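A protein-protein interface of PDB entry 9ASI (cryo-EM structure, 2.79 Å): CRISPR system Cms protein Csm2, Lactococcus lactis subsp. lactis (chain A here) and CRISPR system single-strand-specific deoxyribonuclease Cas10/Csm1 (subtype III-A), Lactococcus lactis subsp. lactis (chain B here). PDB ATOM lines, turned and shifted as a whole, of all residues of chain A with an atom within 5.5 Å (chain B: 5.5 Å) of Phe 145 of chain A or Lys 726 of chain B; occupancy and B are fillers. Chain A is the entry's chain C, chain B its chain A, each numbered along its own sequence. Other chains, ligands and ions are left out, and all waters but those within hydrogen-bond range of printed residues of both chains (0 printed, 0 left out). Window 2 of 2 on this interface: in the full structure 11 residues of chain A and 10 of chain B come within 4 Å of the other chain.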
ATOM      1  N   ALA A 141     -21.261  15.967  29.577  1.00  0.00           N
ATOM      2  CA  ALA A 141     -21.748  17.154  28.883  1.00  0.00           C
ATOM      3  C   ALA A 141     -20.614  18.103  28.527  1.00  0.00           C
ATOM      4  O   ALA A 141     -20.667  18.769  27.488  1.00  0.00           O
ATOM      5  CB  ALA A 141     -22.784  17.869  29.748  1.00  0.00           C
ATOM      6  N   TYR A 142     -19.596  18.191  29.382  1.00  0.00           N
ATOM      7  CA  TYR A 142     -18.458  19.067  29.138  1.00  0.00           C
ATOM      8  C   TYR A 142     -17.420  18.444  28.218  1.00  0.00           C
ATOM      9  O   TYR A 142     -16.737  19.173  27.491  1.00  0.00           O
ATOM     10  CB  TYR A 142     -17.805  19.461  30.461  1.00  0.00           C
ATOM     11  CG  TYR A 142     -18.504  20.605  31.149  1.00  0.00           C
ATOM     12  CD1 TYR A 142     -18.694  21.814  30.501  1.00  0.00           C
ATOM     13  CD2 TYR A 142     -18.981  20.474  32.443  1.00  0.00           C
ATOM     14  CE1 TYR A 142     -19.331  22.861  31.127  1.00  0.00           C
ATOM     15  CE2 TYR A 142     -19.624  21.515  33.076  1.00  0.00           C
ATOM     16  CZ  TYR A 142     -19.796  22.708  32.414  1.00  0.00           C
ATOM     17  OH  TYR A 142     -20.436  23.749  33.045  1.00  0.00           O
ATOM     18  N   PHE A 143     -17.271  17.117  28.246  1.00  0.00           N
ATOM     19  CA  PHE A 143     -16.518  16.456  27.186  1.00  0.00           C
ATOM     20  C   PHE A 143     -17.119  16.794  25.831  1.00  0.00           C
ATOM     21  O   PHE A 143     -16.395  17.057  24.865  1.00  0.00           O
ATOM     22  CB  PHE A 143     -16.497  14.943  27.403  1.00  0.00           C
ATOM     23  CG  PHE A 143     -15.636  14.202  26.418  1.00  0.00           C
ATOM     24  CD1 PHE A 143     -16.163  13.738  25.224  1.00  0.00           C
ATOM     25  CD2 PHE A 143     -14.296  13.977  26.684  1.00  0.00           C
ATOM     26  CE1 PHE A 143     -15.373  13.058  24.319  1.00  0.00           C
ATOM     27  CE2 PHE A 143     -13.501  13.300  25.783  1.00  0.00           C
ATOM     28  CZ  PHE A 143     -14.040  12.840  24.598  1.00  0.00           C
ATOM     29  N   LYS A 144     -18.445  16.794  25.749  1.00  0.00           N
ATOM     30  CA  LYS A 144     -19.118  17.395  24.609  1.00  0.00           C
ATOM     31  C   LYS A 144     -18.925  18.912  24.641  1.00  0.00           C
ATOM     32  O   LYS A 144     -18.795  19.520  25.706  1.00  0.00           O
ATOM     33  CB  LYS A 144     -20.601  17.026  24.626  1.00  0.00           C
ATOM     34  CG  LYS A 144     -21.346  17.273  23.329  1.00  0.00           C
ATOM     35  CD  LYS A 144     -22.553  16.349  23.224  1.00  0.00           C
ATOM     36  CE  LYS A 144     -23.498  16.535  24.402  1.00  0.00           C
ATOM     37  NZ  LYS A 144     -24.705  15.661  24.322  1.00  0.00           N
ATOM     38  N   PHE A 145     -18.879  19.518  23.453  1.00  0.00           N
ATOM     39  CA  PHE A 145     -18.634  20.931  23.164  1.00  0.00           C
ATOM     40  C   PHE A 145     -17.151  21.307  23.294  1.00  0.00           C
ATOM     41  O   PHE A 145     -16.761  22.375  22.820  1.00  0.00           O
ATOM     42  CB  PHE A 145     -19.479  21.879  24.044  1.00  0.00           C
ATOM     43  CG  PHE A 145     -19.092  23.332  23.945  1.00  0.00           C
ATOM     44  CD1 PHE A 145     -19.194  24.017  22.745  1.00  0.00           C
ATOM     45  CD2 PHE A 145     -18.607  24.006  25.052  1.00  0.00           C
ATOM     46  CE1 PHE A 145     -18.830  25.345  22.656  1.00  0.00           C
ATOM     47  CE2 PHE A 145     -18.244  25.335  24.970  1.00  0.00           C
ATOM     48  CZ  PHE A 145     -18.355  26.007  23.770  1.00  0.00           C
ATOM     49  N   TYR A 146     -16.295  20.444  23.835  1.00  0.00           N
ATOM     50  CA  TYR A 146     -14.853  20.657  23.765  1.00  0.00           C
ATOM     51  C   TYR A 146     -14.188  19.767  22.728  1.00  0.00           C
ATOM     52  O   TYR A 146     -13.390  20.248  21.919  1.00  0.00           O
ATOM     53  CB  TYR A 146     -14.196  20.442  25.137  1.00  0.00           C
ATOM     54  CG  TYR A 146     -14.423  21.570  26.119  1.00  0.00           C
ATOM     55  CD1 TYR A 146     -14.868  22.813  25.688  1.00  0.00           C
ATOM     56  CD2 TYR A 146     -14.178  21.398  27.474  1.00  0.00           C
ATOM     57  CE1 TYR A 146     -15.071  23.849  26.581  1.00  0.00           C
ATOM     58  CE2 TYR A 146     -14.378  22.428  28.375  1.00  0.00           C
ATOM     59  CZ  TYR A 146     -14.825  23.651  27.923  1.00  0.00           C
ATOM     60  OH  TYR A 146     -15.025  24.678  28.816  1.00  0.00           O
ATOM     61  N   GLY A 147     -14.510  18.479  22.721  1.00  0.00           N
ATOM     62  CA  GLY A 147     -13.929  17.572  21.757  1.00  0.00           C
ATOM     63  C   GLY A 147     -14.856  17.295  20.594  1.00  0.00           C
ATOM     64  O   GLY A 147     -15.007  18.127  19.695  1.00  0.00           O
ATOM     65  N   THR B 716     -26.945  23.666  28.847  1.00  0.00           N
ATOM     66  CA  THR B 716     -26.714  24.625  27.773  1.00  0.00           C
ATOM     67  C   THR B 716     -25.356  24.392  27.129  1.00  0.00           C
ATOM     68  O   THR B 716     -25.212  24.495  25.906  1.00  0.00           O
ATOM     69  CB  THR B 716     -26.817  26.054  28.310  1.00  0.00           C
ATOM     70  OG1 THR B 716     -28.066  26.221  28.992  1.00  0.00           O
ATOM     71  CG2 THR B 716     -26.738  27.059  27.171  1.00  0.00           C
ATOM     72  N   LEU B 717     -24.346  24.077  27.944  1.00  0.00           N
ATOM     73  CA  LEU B 717     -23.045  23.701  27.396  1.00  0.00           C
ATOM     74  C   LEU B 717     -23.148  22.427  26.564  1.00  0.00           C
ATOM     75  O   LEU B 717     -22.517  22.309  25.508  1.00  0.00           O
ATOM     76  CB  LEU B 717     -22.036  23.518  28.528  1.00  0.00           C
ATOM     77  CG  LEU B 717     -21.193  24.719  28.970  1.00  0.00           C
ATOM     78  CD1 LEU B 717     -20.207  25.134  27.894  1.00  0.00           C
ATOM     79  CD2 LEU B 717     -22.065  25.889  29.370  1.00  0.00           C
ATOM     80  N   SER B 718     -23.942  21.463  27.035  1.00  0.00           N
ATOM     81  CA  SER B 718     -24.081  20.179  26.355  1.00  0.00           C
ATOM     82  C   SER B 718     -24.731  20.333  24.988  1.00  0.00           C
ATOM     83  O   SER B 718     -24.356  19.642  24.035  1.00  0.00           O
ATOM     84  CB  SER B 718     -24.897  19.224  27.225  1.00  0.00           C
ATOM     85  OG  SER B 718     -25.224  18.039  26.525  1.00  0.00           O
ATOM     86  N   ARG B 719     -25.721  21.218  24.879  1.00  0.00           N
ATOM     87  CA  ARG B 719     -26.443  21.395  23.623  1.00  0.00           C
ATOM     88  C   ARG B 719     -25.479  21.747  22.497  1.00  0.00           C
ATOM     89  O   ARG B 719     -24.908  22.841  22.484  1.00  0.00           O
ATOM     90  CB  ARG B 719     -27.511  22.480  23.763  1.00  0.00           C
ATOM     91  CG  ARG B 719     -28.676  22.110  24.662  1.00  0.00           C
ATOM     92  CD  ARG B 719     -29.512  21.000  24.052  1.00  0.00           C
ATOM     93  NE  ARG B 719     -29.144  19.687  24.568  1.00  0.00           N
ATOM     94  CZ  ARG B 719     -29.441  18.540  23.973  1.00  0.00           C
ATOM     95  NH1 ARG B 719     -30.086  18.506  22.820  1.00  0.00           N
ATOM     96  NH2 ARG B 719     -29.078  17.398  24.548  1.00  0.00           N
ATOM     97  N   MET B 720     -25.302  20.832  21.541  1.00  0.00           N
ATOM     98  CA  MET B 720     -24.282  20.980  20.504  1.00  0.00           C
ATOM     99  C   MET B 720     -24.832  20.521  19.161  1.00  0.00           C
ATOM    100  O   MET B 720     -25.021  19.322  18.939  1.00  0.00           O
ATOM    101  CB  MET B 720     -23.018  20.201  20.862  1.00  0.00           C
ATOM    102  CG  MET B 720     -22.107  20.954  21.800  1.00  0.00           C
ATOM    103  SD  MET B 720     -21.998  22.695  21.349  1.00  0.00           S
ATOM    104  CE  MET B 720     -21.171  22.588  19.764  1.00  0.00           C
ATOM    105  N   LYS B 723     -25.872  25.733  14.725  1.00  0.00           N
ATOM    106  CA  LYS B 723     -26.778  26.819  15.074  1.00  0.00           C
ATOM    107  C   LYS B 723     -25.974  28.113  15.037  1.00  0.00           C
ATOM    108  O   LYS B 723     -24.910  28.177  14.412  1.00  0.00           O
ATOM    109  CB  LYS B 723     -27.434  26.560  16.441  1.00  0.00           C
ATOM    110  CG  LYS B 723     -26.448  26.238  17.551  1.00  0.00           C
ATOM    111  CD  LYS B 723     -27.040  26.524  18.920  1.00  0.00           C
ATOM    112  CE  LYS B 723     -27.892  25.365  19.406  1.00  0.00           C
ATOM    113  NZ  LYS B 723     -27.944  25.302  20.893  1.00  0.00           N
ATOM    114  N   ILE B 724     -26.487  29.152  15.695  1.00  0.00           N
ATOM    115  CA  ILE B 724     -25.760  30.406  15.881  1.00  0.00           C
ATOM    116  C   ILE B 724     -24.409  30.127  16.530  1.00  0.00           C
ATOM    117  O   ILE B 724     -23.488  30.948  16.454  1.00  0.00           O
ATOM    118  CB  ILE B 724     -26.571  31.401  16.732  1.00  0.00           C
ATOM    119  CG1 ILE B 724     -26.574  30.964  18.200  1.00  0.00           C
ATOM    120  CG2 ILE B 724     -27.991  31.525  16.200  1.00  0.00           C
ATOM    121  CD1 ILE B 724     -27.013  32.038  19.165  1.00  0.00           C
ATOM    122  N   GLY B 725     -24.285  28.966  17.169  1.00  0.00           N
ATOM    123  CA  GLY B 725     -23.082  28.598  17.879  1.00  0.00           C
ATOM    124  C   GLY B 725     -23.310  28.651  19.372  1.00  0.00           C
ATOM    125  O   GLY B 725     -24.428  28.427  19.843  1.00  0.00           O
ATOM    126  N   LYS B 726     -22.258  28.949  20.129  1.00  0.00           N
ATOM    127  CA  LYS B 726     -22.369  29.126  21.571  1.00  0.00           C
ATOM    128  C   LYS B 726     -21.909  30.511  22.005  1.00  0.00           C
ATOM    129  O   LYS B 726     -21.605  30.719  23.182  1.00  0.00           O
ATOM    130  CB  LYS B 726     -21.586  28.036  22.305  1.00  0.00           C
ATOM    131  CG  LYS B 726     -21.960  26.627  21.875  1.00  0.00           C
ATOM    132  CD  LYS B 726     -23.424  26.335  22.158  1.00  0.00           C
ATOM    133  CE  LYS B 726     -23.665  26.104  23.640  1.00  0.00           C
ATOM    134  NZ  LYS B 726     -25.086  25.768  23.931  1.00  0.00           N
ATOM    135  N   THR B 727     -21.840  31.461  21.073  1.00  0.00           N
ATOM    136  CA  THR B 727     -21.518  32.836  21.436  1.00  0.00           C
ATOM    137  C   THR B 727     -22.595  33.418  22.344  1.00  0.00           C
ATOM    138  O   THR B 727     -22.336  33.757  23.504  1.00  0.00           O
ATOM    139  CB  THR B 727     -21.355  33.686  20.175  1.00  0.00           C
ATOM    140  OG1 THR B 727     -22.636  33.898  19.568  1.00  0.00           O
ATOM    141  CG2 THR B 727     -20.440  32.986  19.182  1.00  0.00           C
ATOM    142  N   PHE B 728     -23.821  33.527  21.833  1.00  0.00           N
ATOM    143  CA  PHE B 728     -24.931  33.991  22.656  1.00  0.00           C
ATOM    144  C   PHE B 728     -25.418  32.911  23.614  1.00  0.00           C
ATOM    145  O   PHE B 728     -25.933  33.231  24.692  1.00  0.00           O
ATOM    146  CB  PHE B 728     -26.077  34.469  21.765  1.00  0.00           C
ATOM    147  CG  PHE B 728     -26.977  35.468  22.427  1.00  0.00           C
ATOM    148  CD1 PHE B 728     -26.456  36.617  22.993  1.00  0.00           C
ATOM    149  CD2 PHE B 728     -28.345  35.259  22.485  1.00  0.00           C
ATOM    150  CE1 PHE B 728     -27.278  37.541  23.604  1.00  0.00           C
ATOM    151  CE2 PHE B 728     -29.173  36.178  23.095  1.00  0.00           C
ATOM    152  CZ  PHE B 728     -28.638  37.322  23.654  1.00  0.00           C
ATOM    153  N   ALA B 729     -25.259  31.637  23.247  1.00  0.00           N
ATOM    154  CA  ALA B 729     -25.629  30.553  24.148  1.00  0.00           C
ATOM    155  C   ALA B 729     -24.764  30.530  25.402  1.00  0.00           C
ATOM    156  O   ALA B 729     -25.179  29.960  26.417  1.00  0.00           O
ATOM    157  CB  ALA B 729     -25.545  29.213  23.419  1.00  0.00           C
ATOM    158  N   GLN B 730     -23.571  31.126  25.355  1.00  0.00           N
ATOM    159  CA  GLN B 730     -22.778  31.358  26.554  1.00  0.00           C
ATOM    160  C   GLN B 730     -22.890  32.786  27.067  1.00  0.00           C
ATOM    161  O   GLN B 730     -22.592  33.034  28.239  1.00  0.00           O
ATOM    162  CB  GLN B 730     -21.302  31.031  26.297  1.00  0.00           C
ATOM    163  CG  GLN B 730     -21.031  29.560  26.016  1.00  0.00           C
ATOM    164  CD  GLN B 730     -21.522  28.652  27.122  1.00  0.00           C
ATOM    165  OE1 GLN B 730     -22.451  27.869  26.931  1.00  0.00           O
ATOM    166  NE2 GLN B 730     -20.899  28.756  28.291  1.00  0.00           N
ATOM    167  N   GLU B 731     -23.317  33.727  26.222  1.00  0.00           N
ATOM    168  CA  GLU B 731     -23.645  35.059  26.718  1.00  0.00           C
ATOM    169  C   GLU B 731     -24.825  35.007  27.677  1.00  0.00           C
ATOM    170  O   GLU B 731     -24.912  35.818  28.604  1.00  0.00           O
ATOM    171  CB  GLU B 731     -23.939  36.000  25.548  1.00  0.00           C
ATOM    172  CG  GLU B 731     -24.592  37.321  25.934  1.00  0.00           C
ATOM    173  CD  GLU B 731     -23.591  38.357  26.417  1.00  0.00           C
ATOM    174  OE1 GLU B 731     -22.521  37.969  26.931  1.00  0.00           O
ATOM    175  OE2 GLU B 731     -23.874  39.564  26.275  1.00  0.00           O
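Printed residues of chain B within 4 Å of Ala 141 of chain A: Ser 718. Of the printed residues of chain B, Tyr 142 of chain A touches Leu 717. Phe 143 of chain A touches none of the printed residues of chain B. Phe 145 of chain A touches just these residues of chain B: Leu 717 (3.4 Å), Met 720 (3.4 Å) and Lys 726 (3.5 Å). Tyr 146 of chain A touches none of the printed residues of chain B. Of the printed residues of chain A, Leu 717 of chain B touches Tyr 142 (3.4 Å) and Phe 145 (3.4 Å). Of the printed residues of chain A, Ser 718 of chain B touches Ala 141 and Lys 144. Printed residues of chain A within 4 Å of Met 720 of chain B: Phe 145. Of chain A, only Phe 145 comes within 4 Å of Lys 726 of chain B. The nearest printed residue of chain A that does not touch Lys 726 of chain B is Lys 144 of chain A (8.4 Å).
OG of Ser 718 of chain B sits close to NZ of Lys 144 of chain A, 3.3 Å away.
Hydrophobic or aromatic side chains of chain A within 4 Å of the printed part of chain B: Ala 141, Tyr 142 and Phe 145. Among the printed residues, no Asp or Glu carboxylate lies within 4 Å of a Lys or Arg side-chain nitrogen of the other chain.
Among the printed residues, pairs that only touch across the chains: Ala 141 of chain A with Ser 718 of chain B, Tyr 142 of chain A with Leu 717 of chain B, Phe 145 of chain A with Leu 717 of chain B, Phe 145 of chain A with Met 720 of chain B and Phe 145 of chain A with Lys 726 of chain B.
The backbone carbonyl oxygen (O) of Arg 719 of chain B sits at hydrogen-bond distance from the side-chain amino group (NZ) of Lys 726 of chain B, at 3.3 Å.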
